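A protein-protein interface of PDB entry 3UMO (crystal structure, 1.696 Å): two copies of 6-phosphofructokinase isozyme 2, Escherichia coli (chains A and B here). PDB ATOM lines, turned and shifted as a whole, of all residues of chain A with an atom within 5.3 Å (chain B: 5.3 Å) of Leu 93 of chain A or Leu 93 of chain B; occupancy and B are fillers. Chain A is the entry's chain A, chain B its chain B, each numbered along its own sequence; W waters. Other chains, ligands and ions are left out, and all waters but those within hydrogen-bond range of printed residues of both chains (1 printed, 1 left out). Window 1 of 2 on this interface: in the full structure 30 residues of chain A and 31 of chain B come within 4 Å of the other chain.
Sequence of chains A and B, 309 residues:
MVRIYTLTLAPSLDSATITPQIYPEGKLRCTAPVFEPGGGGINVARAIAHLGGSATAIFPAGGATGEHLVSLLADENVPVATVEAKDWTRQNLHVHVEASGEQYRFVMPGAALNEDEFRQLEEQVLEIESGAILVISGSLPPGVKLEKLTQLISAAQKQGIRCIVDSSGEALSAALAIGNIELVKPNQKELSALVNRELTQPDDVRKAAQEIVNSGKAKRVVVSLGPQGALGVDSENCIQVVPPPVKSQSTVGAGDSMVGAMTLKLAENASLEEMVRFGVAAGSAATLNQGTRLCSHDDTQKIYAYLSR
OE1 of Gln 91 of chain A lies close to OE1 of Gln 91 of chain B.
O of Leu 93 of chain B sits at hydrogen-bond distance from N of Phe 106 of chain B. OG of Ser 15 of chain A sits at hydrogen-bond distance from NE2 of Gln 91 of chain A. The backbone carbonyl oxygen of Val 95 of chain B is in hydrogen-bond range of the backbone NH of Tyr 104 of chain B, 2.7 Å away. O of Leu 93 of chain A is in hydrogen-bond range of N of Phe 106 of chain A (2.9 Å). N of Val 95 of chain A sits at hydrogen-bond distance from O of Tyr 104 of chain A, 2.8 Å away. The side-chain amide oxygen (OD1) of Asn 92 of chain A sits at hydrogen-bond distance from the backbone NH (N) of Met 108 of chain A (2.8 Å).
Leu 93 of chain B touches Leu 93 of chain A. Leu 93 of chain A touches Phe 106 of chain B. Leu 93 of chain A touches Met 108 of chain B (CD1 to CE, 3.98 Å). CG2 of Val 95 of chain A touches CD2 of Phe 106 of chain B, 3.9 Å away. Phe 106 of chain A touches Leu 93 of chain B (CB to CD2, 3.9 Å). Phe 106 of chain A touches Val 95 of chain B. CZ of Phe 106 of chain B touches CZ of Phe 106 of chain A (3.5 Å). Met 108 of chain A touches Leu 93 of chain B (CE to CD1, 3.8 Å).
Leu 93 of chain A touches just these residues of chain B: Leu 93 (3.7 Å), Phe 106 (3.9 Å) and Met 108 (3.98 Å). Of the printed residues of chain B, Val 95 of chain A touches Phe 106. Printed residues of chain B within 4 Å of Phe 106 of chain A: Leu 93 (3.9 Å), Val 95 (3.9 Å) and Phe 106 (3.5 Å). Ala 16 of chain B touches none of the printed residues of chain A. Asn 92 of chain B touches none of the printed residues of chain A. Leu 93 of chain B touches just these residues of chain A: Leu 93 (3.7 Å), Phe 106 (3.9 Å) and Met 108 (3.8 Å). Printed residues of chain A within 4 Å of Val 95 of chain B: Phe 106 (3.9 Å). Printed residues of chain A within 4 Å of Met 108 of chain B: Leu 93. The nearest printed residue of chain A that does not touch Leu 93 of chain B is Asn 92 of chain A (6.4 Å). The nearest printed residue of chain B that does not touch Gln 91 of chain A is Leu 93 of chain B (6.5 Å).
Of the 13 printed residues of chain B, 5 touch a printed residue of chain A. Of the 13 printed residues of chain A, 5 touch a printed residue of chain B. Printed residues of chain A that touch a printed residue of chain B: Gln 91, Leu 93, Val 95, Phe 106 and Met 108. Among the printed residues, no Asp or Glu carboxylate lies within 4 Å of a Lys or Arg side-chain nitrogen of the other chain.
Leu 93 of chain A touches its own counterpart, Leu 93 of chain B. Leu 93 of chain A touches Phe 106 of chain B, and with the chains exchanged Phe 106 of chain A touches Leu 93 of chain B. Leu 93 of chain A touches Met 108 of chain B, and with the chains exchanged Met 108 of chain A touches Leu 93 of chain B. Phe 106 of chain B touches its own counterpart, Phe 106 of chain A. 13 positions are printed for both chains.
Water W1 bridges N of Gln 91 of chain A and NE2 of Gln 91 of chain B.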
ATOM      1  N   ASP A  14     -16.114  22.931 -26.346  1.00  0.00           N
ATOM      2  CA  ASP A  14     -14.705  23.126 -26.035  1.00  0.00           C
ATOM      3  C   ASP A  14     -14.422  24.537 -25.544  1.00  0.00           C
ATOM      4  O   ASP A  14     -15.030  25.506 -26.004  1.00  0.00           O
ATOM      5  CB  ASP A  14     -13.825  22.784 -27.245  1.00  0.00           C
ATOM      6  CG  ASP A  14     -13.909  21.320 -27.630  1.00  0.00           C
ATOM      7  OD1 ASP A  14     -14.298  20.501 -26.769  1.00  0.00           O
ATOM      8  OD2 ASP A  14     -13.585  20.988 -28.788  1.00  0.00           O
ATOM      9  N   SER A  15     -13.507  24.638 -24.588  1.00  0.00           N
ATOM     10  CA  SER A  15     -13.067  25.929 -24.083  1.00  0.00           C
ATOM     11  C   SER A  15     -11.688  26.219 -24.640  1.00  0.00           C
ATOM     12  O   SER A  15     -10.794  25.385 -24.541  1.00  0.00           O
ATOM     13  CB  SER A  15     -12.991  25.918 -22.554  1.00  0.00           C
ATOM     14  OG  SER A  15     -14.275  25.864 -21.968  1.00  0.00           O
ATOM     15  N   ALA A  16     -11.514  27.394 -25.234  1.00  0.00           N
ATOM     16  CA  ALA A  16     -10.189  27.826 -25.662  1.00  0.00           C
ATOM     17  C   ALA A  16      -9.746  28.963 -24.753  1.00  0.00           C
ATOM     18  O   ALA A  16     -10.420  29.993 -24.652  1.00  0.00           O
ATOM     19  CB  ALA A  16     -10.205  28.284 -27.111  1.00  0.00           C
ATOM     20  N   THR A  17      -8.616  28.770 -24.085  1.00  0.00           N
ATOM     21  CA  THR A  17      -8.120  29.774 -23.156  1.00  0.00           C
ATOM     22  C   THR A  17      -6.652  30.100 -23.404  1.00  0.00           C
ATOM     23  O   THR A  17      -5.955  29.379 -24.134  1.00  0.00           O
ATOM     24  CB  THR A  17      -8.316  29.323 -21.694  1.00  0.00           C
ATOM     25  OG1 THR A  17      -7.939  30.386 -20.813  1.00  0.00           O
ATOM     26  CG2 THR A  17      -7.476  28.085 -21.389  1.00  0.00           C
ATOM     27  N   GLN A  91     -16.725  18.978 -21.801  1.00  0.00           N
ATOM     28  CA  GLN A  91     -15.869  20.038 -22.320  1.00  0.00           C
ATOM     29  C   GLN A  91     -14.417  19.594 -22.450  1.00  0.00           C
ATOM     30  O   GLN A  91     -13.844  19.051 -21.500  1.00  0.00           O
ATOM     31  CB  GLN A  91     -15.908  21.247 -21.386  1.00  0.00           C
ATOM     32  CG  GLN A  91     -17.297  21.786 -21.072  1.00  0.00           C
ATOM     33  CD  GLN A  91     -17.266  23.273 -20.752  1.00  0.00           C
ATOM     34  OE1 GLN A  91     -17.731  23.707 -19.698  1.00  0.00           O
ATOM     35  NE2 GLN A  91     -16.710  24.064 -21.668  1.00  0.00           N
ATOM     36  N   ASN A  92     -13.823  19.823 -23.621  1.00  0.00           N
ATOM     37  CA  ASN A  92     -12.377  19.670 -23.764  1.00  0.00           C
ATOM     38  C   ASN A  92     -11.709  21.034 -23.637  1.00  0.00           C
ATOM     39  O   ASN A  92     -12.369  22.065 -23.773  1.00  0.00           O
ATOM     40  CB  ASN A  92     -12.006  18.998 -25.090  1.00  0.00           C
ATOM     41  CG  ASN A  92     -12.474  17.567 -25.160  1.00  0.00           C
ATOM     42  OD1 ASN A  92     -12.581  16.896 -24.136  1.00  0.00           O
ATOM     43  ND2 ASN A  92     -12.769  17.093 -26.364  1.00  0.00           N
ATOM     44  N   LEU A  93     -10.409  21.041 -23.366  1.00  0.00           N
ATOM     45  CA  LEU A  93      -9.707  22.296 -23.125  1.00  0.00           C
ATOM     46  C   LEU A  93      -8.541  22.506 -24.080  1.00  0.00           C
ATOM     47  O   LEU A  93      -7.663  21.644 -24.204  1.00  0.00           O
ATOM     48  CB  LEU A  93      -9.208  22.376 -21.679  1.00  0.00           C
ATOM     49  CG  LEU A  93      -8.565  23.709 -21.274  1.00  0.00           C
ATOM     50  CD1 LEU A  93      -9.570  24.851 -21.351  1.00  0.00           C
ATOM     51  CD2 LEU A  93      -7.929  23.637 -19.884  1.00  0.00           C
ATOM     52  N   HIS A  94      -8.541  23.667 -24.734  1.00  0.00           N
ATOM     53  CA  HIS A  94      -7.463  24.087 -25.619  1.00  0.00           C
ATOM     54  C   HIS A  94      -6.750  25.242 -24.934  1.00  0.00           C
ATOM     55  O   HIS A  94      -7.365  26.268 -24.640  1.00  0.00           O
ATOM     56  CB  HIS A  94      -8.043  24.553 -26.961  1.00  0.00           C
ATOM     57  CG  HIS A  94      -7.021  25.061 -27.933  1.00  0.00           C
ATOM     58  ND1 HIS A  94      -6.532  26.352 -27.891  1.00  0.00           N
ATOM     59  CD2 HIS A  94      -6.417  24.463 -28.985  1.00  0.00           C
ATOM     60  CE1 HIS A  94      -5.659  26.518 -28.872  1.00  0.00           C
ATOM     61  NE2 HIS A  94      -5.573  25.388 -29.549  1.00  0.00           N
ATOM     62  N   VAL A  95      -5.456  25.084 -24.674  1.00  0.00           N
ATOM     63  CA  VAL A  95      -4.697  26.139 -24.007  1.00  0.00           C
ATOM     64  C   VAL A  95      -3.600  26.700 -24.900  1.00  0.00           C
ATOM     65  O   VAL A  95      -2.703  25.971 -25.329  1.00  0.00           O
ATOM     66  CB  VAL A  95      -4.034  25.626 -22.712  1.00  0.00           C
ATOM     67  CG1 VAL A  95      -3.324  26.773 -21.984  1.00  0.00           C
ATOM     68  CG2 VAL A  95      -5.053  24.962 -21.810  1.00  0.00           C
ATOM     69  N   TYR A 104      -1.876  23.479 -26.273  1.00  0.00           N
ATOM     70  CA  TYR A 104      -2.030  22.210 -25.574  1.00  0.00           C
ATOM     71  C   TYR A 104      -3.483  21.801 -25.616  1.00  0.00           C
ATOM     72  O   TYR A 104      -4.377  22.618 -25.409  1.00  0.00           O
ATOM     73  CB  TYR A 104      -1.527  22.333 -24.136  1.00  0.00           C
ATOM     74  CG  TYR A 104      -0.020  22.468 -24.061  1.00  0.00           C
ATOM     75  CD1 TYR A 104       0.788  21.355 -23.847  1.00  0.00           C
ATOM     76  CD2 TYR A 104       0.595  23.703 -24.240  1.00  0.00           C
ATOM     77  CE1 TYR A 104       2.159  21.468 -23.793  1.00  0.00           C
ATOM     78  CE2 TYR A 104       1.972  23.827 -24.189  1.00  0.00           C
ATOM     79  CZ  TYR A 104       2.748  22.707 -23.968  1.00  0.00           C
ATOM     80  OH  TYR A 104       4.116  22.836 -23.915  1.00  0.00           O
ATOM     81  N   ARG A 105      -3.727  20.523 -25.876  1.00  0.00           N
ATOM     82  CA  ARG A 105      -5.083  20.072 -26.144  1.00  0.00           C
ATOM     83  C   ARG A 105      -5.421  18.904 -25.250  1.00  0.00           C
ATOM     84  O   ARG A 105      -4.899  17.810 -25.430  1.00  0.00           O
ATOM     85  CB  ARG A 105      -5.205  19.664 -27.609  1.00  0.00           C
ATOM     86  CG  ARG A 105      -4.874  20.790 -28.581  1.00  0.00           C
ATOM     87  CD  ARG A 105      -4.500  20.230 -29.945  1.00  0.00           C
ATOM     88  NE  ARG A 105      -5.641  19.605 -30.604  1.00  0.00           N
ATOM     89  CZ  ARG A 105      -5.558  18.823 -31.682  1.00  0.00           C
ATOM     90  NH1 ARG A 105      -4.383  18.546 -32.232  1.00  0.00           N
ATOM     91  NH2 ARG A 105      -6.659  18.309 -32.207  1.00  0.00           N
ATOM     92  N   PHE A 106      -6.296  19.135 -24.281  1.00  0.00           N
ATOM     93  CA  PHE A 106      -6.667  18.080 -23.346  1.00  0.00           C
ATOM     94  C   PHE A 106      -8.019  17.517 -23.738  1.00  0.00           C
ATOM     95  O   PHE A 106      -9.040  18.204 -23.659  1.00  0.00           O
ATOM     96  CB  PHE A 106      -6.651  18.623 -21.916  1.00  0.00           C
ATOM     97  CG  PHE A 106      -5.330  19.219 -21.535  1.00  0.00           C
ATOM     98  CD1 PHE A 106      -5.086  20.575 -21.718  1.00  0.00           C
ATOM     99  CD2 PHE A 106      -4.303  18.419 -21.060  1.00  0.00           C
ATOM    100  CE1 PHE A 106      -3.854  21.129 -21.405  1.00  0.00           C
ATOM    101  CE2 PHE A 106      -3.065  18.965 -20.736  1.00  0.00           C
ATOM    102  CZ  PHE A 106      -2.840  20.327 -20.910  1.00  0.00           C
ATOM    103  N   MET A 108     -10.897  14.813 -23.280  1.00  0.00           N
ATOM    104  CA  MET A 108     -11.535  13.893 -22.347  1.00  0.00           C
ATOM    105  C   MET A 108     -12.725  13.232 -23.034  1.00  0.00           C
ATOM    106  O   MET A 108     -13.128  13.666 -24.116  1.00  0.00           O
ATOM    107  CB  MET A 108     -11.952  14.649 -21.084  1.00  0.00           C
ATOM    108  CG  MET A 108     -10.795  14.864 -20.134  1.00  0.00           C
ATOM    109  SD  MET A 108     -11.146  16.079 -18.858  1.00  0.00           S
ATOM    110  CE  MET A 108     -11.176  17.578 -19.853  1.00  0.00           C
ATOM    111  N   ASP B  14     -14.514  21.223 -10.448  1.00  0.00           N
ATOM    112  CA  ASP B  14     -13.223  20.949 -11.062  1.00  0.00           C
ATOM    113  C   ASP B  14     -13.120  19.530 -11.602  1.00  0.00           C
ATOM    114  O   ASP B  14     -13.729  18.606 -11.068  1.00  0.00           O
ATOM    115  CB  ASP B  14     -12.092  21.254 -10.080  1.00  0.00           C
ATOM    116  CG  ASP B  14     -12.003  22.729  -9.753  1.00  0.00           C
ATOM    117  OD1 ASP B  14     -12.619  23.528 -10.491  1.00  0.00           O
ATOM    118  OD2 ASP B  14     -11.319  23.091  -8.772  1.00  0.00           O
ATOM    119  N   SER B  15     -12.373  19.377 -12.691  1.00  0.00           N
ATOM    120  CA  SER B  15     -12.126  18.064 -13.269  1.00  0.00           C
ATOM    121  C   SER B  15     -10.684  17.653 -13.043  1.00  0.00           C
ATOM    122  O   SER B  15      -9.755  18.404 -13.362  1.00  0.00           O
ATOM    123  CB  SER B  15     -12.431  18.061 -14.770  1.00  0.00           C
ATOM    124  OG  SER B  15     -13.819  18.166 -15.008  1.00  0.00           O
ATOM    125  N   ALA B  16     -10.499  16.460 -12.489  1.00  0.00           N
ATOM    126  CA  ALA B  16      -9.167  15.902 -12.314  1.00  0.00           C
ATOM    127  C   ALA B  16      -9.001  14.744 -13.283  1.00  0.00           C
ATOM    128  O   ALA B  16      -9.751  13.765 -13.240  1.00  0.00           O
ATOM    129  CB  ALA B  16      -8.964  15.430 -10.882  1.00  0.00           C
ATOM    130  N   THR B  17      -8.013  14.855 -14.157  1.00  0.00           N
ATOM    131  CA  THR B  17      -7.796  13.835 -15.172  1.00  0.00           C
ATOM    132  C   THR B  17      -6.329  13.429 -15.257  1.00  0.00           C
ATOM    133  O   THR B  17      -5.451  14.106 -14.703  1.00  0.00           O
ATOM    134  CB  THR B  17      -8.290  14.317 -16.539  1.00  0.00           C
ATOM    135  OG1 THR B  17      -8.119  13.271 -17.497  1.00  0.00           O
ATOM    136  CG2 THR B  17      -7.519  15.570 -16.986  1.00  0.00           C
ATOM    137  N   GLN B  91     -15.803  25.234 -14.781  1.00  0.00           N
ATOM    138  CA  GLN B  91     -14.918  24.127 -14.464  1.00  0.00           C
ATOM    139  C   GLN B  91     -13.464  24.505 -14.697  1.00  0.00           C
ATOM    140  O   GLN B  91     -13.110  25.032 -15.756  1.00  0.00           O
ATOM    141  CB  GLN B  91     -15.267  22.922 -15.338  1.00  0.00           C
ATOM    142  CG  GLN B  91     -16.748  22.580 -15.350  1.00  0.00           C
ATOM    143  CD  GLN B  91     -17.083  21.486 -16.345  1.00  0.00           C
ATOM    144  OE1 GLN B  91     -17.542  21.760 -17.458  1.00  0.00           O
ATOM    145  NE2 GLN B  91     -16.857  20.237 -15.948  1.00  0.00           N
ATOM    146  N   ASN B  92     -12.633  24.253 -13.692  1.00  0.00           N
ATOM    147  CA  ASN B  92     -11.189  24.298 -13.858  1.00  0.00           C
ATOM    148  C   ASN B  92     -10.667  22.887 -14.084  1.00  0.00           C
ATOM    149  O   ASN B  92     -11.348  21.909 -13.774  1.00  0.00           O
ATOM    150  CB  ASN B  92     -10.518  24.912 -12.632  1.00  0.00           C
ATOM    151  CG  ASN B  92     -10.876  26.377 -12.447  1.00  0.00           C
ATOM    152  OD1 ASN B  92     -11.091  27.089 -13.419  1.00  0.00           O
ATOM    153  ND2 ASN B  92     -10.960  26.819 -11.196  1.00  0.00           N
ATOM    154  N   LEU B  93      -9.452  22.790 -14.611  1.00  0.00           N
ATOM    155  CA  LEU B  93      -8.890  21.502 -14.966  1.00  0.00           C
ATOM    156  C   LEU B  93      -7.568  21.223 -14.254  1.00  0.00           C
ATOM    157  O   LEU B  93      -6.647  22.047 -14.264  1.00  0.00           O
ATOM    158  CB  LEU B  93      -8.690  21.408 -16.482  1.00  0.00           C
ATOM    159  CG  LEU B  93      -8.248  20.050 -17.029  1.00  0.00           C
ATOM    160  CD1 LEU B  93      -9.310  18.980 -16.806  1.00  0.00           C
ATOM    161  CD2 LEU B  93      -7.888  20.157 -18.516  1.00  0.00           C
ATOM    162  N   HIS B  94      -7.492  20.038 -13.655  1.00  0.00           N
ATOM    163  CA  HIS B  94      -6.286  19.533 -13.009  1.00  0.00           C
ATOM    164  C   HIS B  94      -5.827  18.316 -13.795  1.00  0.00           C
ATOM    165  O   HIS B  94      -6.566  17.333 -13.934  1.00  0.00           O
ATOM    166  CB  HIS B  94      -6.590  19.138 -11.552  1.00  0.00           C
ATOM    167  CG  HIS B  94      -5.416  18.561 -10.816  1.00  0.00           C
ATOM    168  ND1 HIS B  94      -5.094  17.220 -10.861  1.00  0.00           N
ATOM    169  CD2 HIS B  94      -4.500  19.139 -10.003  1.00  0.00           C
ATOM    170  CE1 HIS B  94      -4.023  17.000 -10.114  1.00  0.00           C
ATOM    171  NE2 HIS B  94      -3.644  18.149  -9.584  1.00  0.00           N
ATOM    172  N   VAL B  95      -4.614  18.383 -14.331  1.00  0.00           N
ATOM    173  CA  VAL B  95      -4.089  17.290 -15.138  1.00  0.00           C
ATOM    174  C   VAL B  95      -2.871  16.665 -14.482  1.00  0.00           C
ATOM    175  O   VAL B  95      -1.878  17.349 -14.225  1.00  0.00           O
ATOM    176  CB  VAL B  95      -3.668  17.774 -16.539  1.00  0.00           C
ATOM    177  CG1 VAL B  95      -3.179  16.592 -17.404  1.00  0.00           C
ATOM    178  CG2 VAL B  95      -4.814  18.493 -17.219  1.00  0.00           C
ATOM    179  N   TYR B 104      -0.674  19.723 -13.559  1.00  0.00           N
ATOM    180  CA  TYR B 104      -0.883  21.022 -14.178  1.00  0.00           C
ATOM    181  C   TYR B 104      -2.271  21.502 -13.828  1.00  0.00           C
ATOM    182  O   TYR B 104      -3.229  20.724 -13.836  1.00  0.00           O
ATOM    183  CB  TYR B 104      -0.705  20.928 -15.694  1.00  0.00           C
ATOM    184  CG  TYR B 104       0.730  20.665 -16.090  1.00  0.00           C
ATOM    185  CD1 TYR B 104       1.569  21.707 -16.456  1.00  0.00           C
ATOM    186  CD2 TYR B 104       1.260  19.380 -16.059  1.00  0.00           C
ATOM    187  CE1 TYR B 104       2.887  21.480 -16.801  1.00  0.00           C
ATOM    188  CE2 TYR B 104       2.585  19.143 -16.402  1.00  0.00           C
ATOM    189  CZ  TYR B 104       3.391  20.202 -16.771  1.00  0.00           C
ATOM    190  OH  TYR B 104       4.711  19.997 -17.113  1.00  0.00           O
ATOM    191  N   ARG B 105      -2.385  22.790 -13.520  1.00  0.00           N
ATOM    192  CA  ARG B 105      -3.638  23.320 -13.010  1.00  0.00           C
ATOM    193  C   ARG B 105      -4.060  24.533 -13.822  1.00  0.00           C
ATOM    194  O   ARG B 105      -3.401  25.575 -13.784  1.00  0.00           O
ATOM    195  CB  ARG B 105      -3.464  23.729 -11.544  1.00  0.00           C
ATOM    196  CG  ARG B 105      -2.905  22.639 -10.656  1.00  0.00           C
ATOM    197  CD  ARG B 105      -2.205  23.238  -9.451  1.00  0.00           C
ATOM    198  NE  ARG B 105      -3.126  23.858  -8.502  1.00  0.00           N
ATOM    199  CZ  ARG B 105      -2.742  24.588  -7.455  1.00  0.00           C
ATOM    200  NH1 ARG B 105      -1.455  24.801  -7.219  1.00  0.00           N
ATOM    201  NH2 ARG B 105      -3.652  25.095  -6.632  1.00  0.00           N
ATOM    202  N   PHE B 106      -5.154  24.396 -14.562  1.00  0.00           N
ATOM    203  CA  PHE B 106      -5.624  25.483 -15.404  1.00  0.00           C
ATOM    204  C   PHE B 106      -6.825  26.144 -14.748  1.00  0.00           C
ATOM    205  O   PHE B 106      -7.900  25.543 -14.622  1.00  0.00           O
ATOM    206  CB  PHE B 106      -5.930  24.960 -16.811  1.00  0.00           C
ATOM    207  CG  PHE B 106      -4.757  24.254 -17.440  1.00  0.00           C
ATOM    208  CD1 PHE B 106      -4.619  22.879 -17.329  1.00  0.00           C
ATOM    209  CD2 PHE B 106      -3.772  24.969 -18.112  1.00  0.00           C
ATOM    210  CE1 PHE B 106      -3.527  22.220 -17.897  1.00  0.00           C
ATOM    211  CE2 PHE B 106      -2.684  24.322 -18.688  1.00  0.00           C
ATOM    212  CZ  PHE B 106      -2.556  22.945 -18.574  1.00  0.00           C
ATOM    213  N   MET B 108      -9.558  29.048 -14.613  1.00  0.00           N
ATOM    214  CA  MET B 108     -10.327  30.024 -15.372  1.00  0.00           C
ATOM    215  C   MET B 108     -11.301  30.748 -14.443  1.00  0.00           C
ATOM    216  O   MET B 108     -11.523  30.303 -13.315  1.00  0.00           O
ATOM    217  CB  MET B 108     -11.066  29.309 -16.506  1.00  0.00           C
ATOM    218  CG  MET B 108     -10.171  29.018 -17.703  1.00  0.00           C
ATOM    219  SD  MET B 108     -10.775  27.709 -18.777  1.00  0.00           S
ATOM    220  CE  MET B 108     -10.504  26.257 -17.747  1.00  0.00           C
HETATM  221  O   HOH W   1     -16.621  18.380 -18.630  1.00  0.00           O
